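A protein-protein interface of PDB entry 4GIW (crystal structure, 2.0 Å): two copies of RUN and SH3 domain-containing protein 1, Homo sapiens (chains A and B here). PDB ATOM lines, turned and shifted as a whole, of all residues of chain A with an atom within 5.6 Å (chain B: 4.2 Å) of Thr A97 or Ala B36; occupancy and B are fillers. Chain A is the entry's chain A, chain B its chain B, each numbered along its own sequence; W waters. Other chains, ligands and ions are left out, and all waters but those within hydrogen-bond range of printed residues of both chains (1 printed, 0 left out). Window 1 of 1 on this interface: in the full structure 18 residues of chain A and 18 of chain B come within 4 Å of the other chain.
Water W1 bridges OD2 of Asp B40 and N of Arg A98.
Among the printed residues, pairs that only touch across the chains: Thr A97 with Ala B36, Leu A135 with Leu B32 and Leu A135 with Val B33.
N of Leu A100 is in hydrogen-bond range of OG1 of Thr A97.
The backbone carbonyl oxygen (O) of Arg A98 is in hydrogen-bond range of the side-chain hydroxyl (OG1) of Thr A102 (2.9 Å).
The side-chain amide oxygen (OE1) of Gln A132 lies within hydrogen-bond range of the side-chain hydroxyl (OG1) of Thr A97.
N of Ser A99 sits close to OG1 of Thr A97 (3.2 Å).
Of the 9 printed residues of chain A, 3 touch a printed residue of chain B.
Printed residues of chain A that touch a printed residue of chain B: Thr A97, Arg A98 and Leu A135.
Of the 9 printed residues of chain B, 4 touch a printed residue of chain A.
Hydrophobic or aromatic side chains of chain B that line the printed part of chain A: Leu B32 and Ala B36.
Among the printed residues, 4 pairs touch across the chains.
Of the printed residues of chain B, Thr A97 touches Ala B36.
Printed residues of chain B within 4 Å of Arg A98: Asp B40.
Printed residues of chain B within 4 Å of Leu A135: Leu B32 and Val B33.
Of the printed residues of chain A, Leu B32 touches Leu A135 (3.5 Å).
Printed residues of chain A within 4 Å of Ala B36: Thr A97.
Gln B37 touches none of the printed residues of chain A.
Of the printed residues of chain A, Asp B40 touches Arg A98 (2.4 Å).
The nearest printed residue of chain B that does not touch Thr A97 is Val B33 (5.1 Å).
The nearest printed residue of chain A that does not touch Ala B36 is Leu A135 (4.01 Å).
The nearest printed residue of chain B that does not touch Arg A98 is Gly B39 (6.5 Å).
No position is printed for both chains.
Of the 4 pairs that touch across the chains among the printed residues, none has its exchanged pair printed and touching as well.
NH1 of Arg A98 lies within salt-bridge range of OD2 of Asp B40 (2.8 Å).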
ATOM      1  N   VAL A  91     -28.464  -6.930   6.335  1.00  0.00           N
ATOM      2  CA  VAL A  91     -27.377  -6.304   7.104  1.00  0.00           C
ATOM      3  C   VAL A  91     -26.014  -6.392   6.423  1.00  0.00           C
ATOM      4  O   VAL A  91     -25.449  -7.477   6.282  1.00  0.00           O
ATOM      5  CB  VAL A  91     -27.321  -6.832   8.582  1.00  0.00           C
ATOM      6  CG1 VAL A  91     -27.253  -8.356   8.640  1.00  0.00           C
ATOM      7  CG2 VAL A  91     -26.156  -6.219   9.333  1.00  0.00           C
ATOM      8  N   THR A  97     -28.308  -1.435  11.688  1.00  0.00           N
ATOM      9  CA  THR A  97     -27.529  -0.720  12.693  1.00  0.00           C
ATOM     10  C   THR A  97     -26.065  -1.146  12.690  1.00  0.00           C
ATOM     11  O   THR A  97     -25.721  -2.229  12.217  1.00  0.00           O
ATOM     12  CB  THR A  97     -28.081  -0.975  14.113  1.00  0.00           C
ATOM     13  OG1 THR A  97     -27.690  -2.284  14.553  1.00  0.00           O
ATOM     14  CG2 THR A  97     -29.585  -0.866  14.122  1.00  0.00           C
ATOM     15  N   ARG A  98     -25.210  -0.292  13.246  1.00  0.00           N
ATOM     16  CA  ARG A  98     -23.813  -0.638  13.498  1.00  0.00           C
ATOM     17  C   ARG A  98     -23.667  -1.912  14.321  1.00  0.00           C
ATOM     18  O   ARG A  98     -22.778  -2.722  14.056  1.00  0.00           O
ATOM     19  CB  ARG A  98     -23.095   0.517  14.191  1.00  0.00           C
ATOM     20  CG  ARG A  98     -22.051   1.197  13.328  1.00  0.00           C
ATOM     21  CD  ARG A  98     -21.782   2.619  13.793  1.00  0.00           C
ATOM     22  NE  ARG A  98     -21.537   2.717  15.233  1.00  0.00           N
ATOM     23  CZ  ARG A  98     -21.522   3.863  15.905  1.00  0.00           C
ATOM     24  NH1 ARG A  98     -21.758   4.991  15.262  1.00  0.00           N
ATOM     25  NH2 ARG A  98     -21.299   3.892  17.215  1.00  0.00           N
ATOM     26  N   SER A  99     -24.546  -2.089  15.310  1.00  0.00           N
ATOM     27  CA  SER A  99     -24.538  -3.280  16.164  1.00  0.00           C
ATOM     28  C   SER A  99     -24.839  -4.544  15.359  1.00  0.00           C
ATOM     29  O   SER A  99     -24.193  -5.578  15.545  1.00  0.00           O
ATOM     30  CB  SER A  99     -25.542  -3.151  17.314  1.00  0.00           C
ATOM     31  OG  SER A  99     -25.724  -1.809  17.739  1.00  0.00           O
ATOM     32  N   LEU A 100     -25.810  -4.448  14.454  1.00  0.00           N
ATOM     33  CA  LEU A 100     -26.159  -5.568  13.584  1.00  0.00           C
ATOM     34  C   LEU A 100     -25.042  -5.936  12.606  1.00  0.00           C
ATOM     35  O   LEU A 100     -24.775  -7.119  12.381  1.00  0.00           O
ATOM     36  CB  LEU A 100     -27.464  -5.280  12.837  1.00  0.00           C
ATOM     37  CG  LEU A 100     -28.742  -5.314  13.680  1.00  0.00           C
ATOM     38  CD1 LEU A 100     -29.948  -4.955  12.833  1.00  0.00           C
ATOM     39  CD2 LEU A 100     -28.935  -6.675  14.316  1.00  0.00           C
ATOM     40  N   GLY A 101     -24.396  -4.920  12.034  1.00  0.00           N
ATOM     41  CA  GLY A 101     -23.318  -5.123  11.064  1.00  0.00           C
ATOM     42  C   GLY A 101     -22.103  -5.834  11.659  1.00  0.00           C
ATOM     43  O   GLY A 101     -21.523  -6.727  11.029  1.00  0.00           O
ATOM     44  N   THR A 102     -21.733  -5.442  12.873  1.00  0.00           N
ATOM     45  CA  THR A 102     -20.624  -6.065  13.581  1.00  0.00           C
ATOM     46  C   THR A 102     -20.914  -7.548  13.799  1.00  0.00           C
ATOM     47  O   THR A 102     -20.087  -8.399  13.474  1.00  0.00           O
ATOM     48  CB  THR A 102     -20.335  -5.348  14.917  1.00  0.00           C
ATOM     49  OG1 THR A 102     -20.234  -3.936  14.685  1.00  0.00           O
ATOM     50  CG2 THR A 102     -19.034  -5.847  15.534  1.00  0.00           C
ATOM     51  N   GLN A 132     -31.017  -7.876  20.337  1.00  0.00           N
ATOM     52  CA  GLN A 132     -31.375  -7.235  19.077  1.00  0.00           C
ATOM     53  C   GLN A 132     -32.364  -8.051  18.236  1.00  0.00           C
ATOM     54  O   GLN A 132     -32.499  -7.793  17.035  1.00  0.00           O
ATOM     55  CB  GLN A 132     -30.125  -6.904  18.253  1.00  0.00           C
ATOM     56  CG  GLN A 132     -29.274  -5.765  18.824  1.00  0.00           C
ATOM     57  CD  GLN A 132     -28.160  -5.357  17.875  1.00  0.00           C
ATOM     58  OE1 GLN A 132     -28.190  -4.267  17.308  1.00  0.00           O
ATOM     59  NE2 GLN A 132     -27.189  -6.238  17.682  1.00  0.00           N
ATOM     60  N   LEU A 135     -35.219  -5.710  17.079  1.00  0.00           N
ATOM     61  CA  LEU A 135     -34.670  -4.762  16.110  1.00  0.00           C
ATOM     62  C   LEU A 135     -34.433  -5.407  14.736  1.00  0.00           C
ATOM     63  O   LEU A 135     -34.740  -4.816  13.696  1.00  0.00           O
ATOM     64  CB  LEU A 135     -33.387  -4.125  16.655  1.00  0.00           C
ATOM     65  CG  LEU A 135     -32.542  -3.256  15.713  1.00  0.00           C
ATOM     66  CD1 LEU A 135     -33.322  -2.040  15.217  1.00  0.00           C
ATOM     67  CD2 LEU A 135     -31.278  -2.824  16.430  1.00  0.00           C
ATOM     68  N   LEU B  32     -38.362   0.780  15.512  1.00  0.00           N
ATOM     69  CA  LEU B  32     -37.159   0.292  16.185  1.00  0.00           C
ATOM     70  C   LEU B  32     -35.853   0.669  15.489  1.00  0.00           C
ATOM     71  O   LEU B  32     -34.866   0.987  16.158  1.00  0.00           O
ATOM     72  CB  LEU B  32     -37.225  -1.225  16.397  1.00  0.00           C
ATOM     73  CG  LEU B  32     -38.290  -1.721  17.379  1.00  0.00           C
ATOM     74  CD1 LEU B  32     -38.108  -3.196  17.664  1.00  0.00           C
ATOM     75  CD2 LEU B  32     -38.260  -0.915  18.679  1.00  0.00           C
ATOM     76  N   VAL B  33     -35.852   0.628  14.157  1.00  0.00           N
ATOM     77  CA  VAL B  33     -34.685   1.022  13.365  1.00  0.00           C
ATOM     78  C   VAL B  33     -34.325   2.486  13.627  1.00  0.00           C
ATOM     79  O   VAL B  33     -33.152   2.820  13.815  1.00  0.00           O
ATOM     80  CB  VAL B  33     -34.894   0.783  11.839  1.00  0.00           C
ATOM     81  CG1 VAL B  33     -33.762   1.426  11.015  1.00  0.00           C
ATOM     82  CG2 VAL B  33     -34.966  -0.710  11.531  1.00  0.00           C
ATOM     83  N   GLN B  34     -35.341   3.347  13.659  1.00  0.00           N
ATOM     84  CA  GLN B  34     -35.141   4.758  13.966  1.00  0.00           C
ATOM     85  C   GLN B  34     -34.715   4.963  15.424  1.00  0.00           C
ATOM     86  O   GLN B  34     -33.907   5.841  15.706  1.00  0.00           O
ATOM     87  CB  GLN B  34     -36.396   5.570  13.652  1.00  0.00           C
ATOM     88  CG  GLN B  34     -36.743   5.662  12.178  1.00  0.00           C
ATOM     89  CD  GLN B  34     -37.985   6.505  11.932  1.00  0.00           C
ATOM     90  OE1 GLN B  34     -38.520   7.121  12.853  1.00  0.00           O
ATOM     91  NE2 GLN B  34     -38.455   6.529  10.687  1.00  0.00           N
ATOM     92  N   LYS B  35     -35.249   4.148  16.340  1.00  0.00           N
ATOM     93  CA  LYS B  35     -34.830   4.201  17.750  1.00  0.00           C
ATOM     94  C   LYS B  35     -33.356   3.845  17.916  1.00  0.00           C
ATOM     95  O   LYS B  35     -32.647   4.465  18.710  1.00  0.00           O
ATOM     96  CB  LYS B  35     -35.687   3.299  18.639  1.00  0.00           C
ATOM     97  CG  LYS B  35     -37.073   3.857  18.947  1.00  0.00           C
ATOM     98  CD  LYS B  35     -37.808   3.024  19.992  1.00  0.00           C
ATOM     99  CE  LYS B  35     -37.602   3.573  21.402  1.00  0.00           C
ATOM    100  NZ  LYS B  35     -38.304   2.736  22.427  1.00  0.00           N
ATOM    101  N   ALA B  36     -32.903   2.853  17.157  1.00  0.00           N
ATOM    102  CA  ALA B  36     -31.488   2.489  17.127  1.00  0.00           C
ATOM    103  C   ALA B  36     -30.610   3.625  16.607  1.00  0.00           C
ATOM    104  O   ALA B  36     -29.504   3.812  17.112  1.00  0.00           O
ATOM    105  CB  ALA B  36     -31.269   1.230  16.310  1.00  0.00           C
ATOM    106  N   GLN B  37     -31.096   4.376  15.614  1.00  0.00           N
ATOM    107  CA  GLN B  37     -30.363   5.531  15.070  1.00  0.00           C
ATOM    108  C   GLN B  37     -30.137   6.582  16.155  1.00  0.00           C
ATOM    109  O   GLN B  37     -29.055   7.167  16.240  1.00  0.00           O
ATOM    110  CB  GLN B  37     -31.096   6.178  13.883  1.00  0.00           C
ATOM    111  CG  GLN B  37     -31.210   5.311  12.617  1.00  0.00           C
ATOM    112  CD  GLN B  37     -32.104   5.929  11.529  1.00  0.00           C
ATOM    113  OE1 GLN B  37     -32.809   6.921  11.753  1.00  0.00           O
ATOM    114  NE2 GLN B  37     -32.075   5.331  10.343  1.00  0.00           N
ATOM    115  N   LEU B  38     -31.161   6.804  16.979  1.00  0.00           N
ATOM    116  CA  LEU B  38     -31.106   7.792  18.056  1.00  0.00           C
ATOM    117  C   LEU B  38     -30.211   7.380  19.225  1.00  0.00           C
ATOM    118  O   LEU B  38     -29.836   8.218  20.044  1.00  0.00           O
ATOM    119  CB  LEU B  38     -32.515   8.127  18.559  1.00  0.00           C
ATOM    120  CG  LEU B  38     -33.418   8.890  17.578  1.00  0.00           C
ATOM    121  CD1 LEU B  38     -34.757   9.200  18.224  1.00  0.00           C
ATOM    122  CD2 LEU B  38     -32.757  10.173  17.119  1.00  0.00           C
ATOM    123  N   GLY B  39     -29.879   6.093  19.290  1.00  0.00           N
ATOM    124  CA  GLY B  39     -28.973   5.559  20.307  1.00  0.00           C
ATOM    125  C   GLY B  39     -27.521   5.473  19.881  1.00  0.00           C
ATOM    126  O   GLY B  39     -26.659   5.127  20.683  1.00  0.00           O
ATOM    127  N   ASP B  40     -27.251   5.778  18.615  1.00  0.00           N
ATOM    128  CA  ASP B  40     -25.907   5.699  18.065  1.00  0.00           C
ATOM    129  C   ASP B  40     -25.247   7.071  18.195  1.00  0.00           C
ATOM    130  O   ASP B  40     -25.727   8.043  17.606  1.00  0.00           O
ATOM    131  CB  ASP B  40     -25.992   5.265  16.598  1.00  0.00           C
ATOM    132  CG  ASP B  40     -24.631   5.066  15.960  1.00  0.00           C
ATOM    133  OD1 ASP B  40     -23.760   5.949  16.112  1.00  0.00           O
ATOM    134  OD2 ASP B  40     -24.432   4.027  15.300  1.00  0.00           O
HETATM  135  O   HOH W   1     -26.280   2.108  14.812  1.00  0.00           O
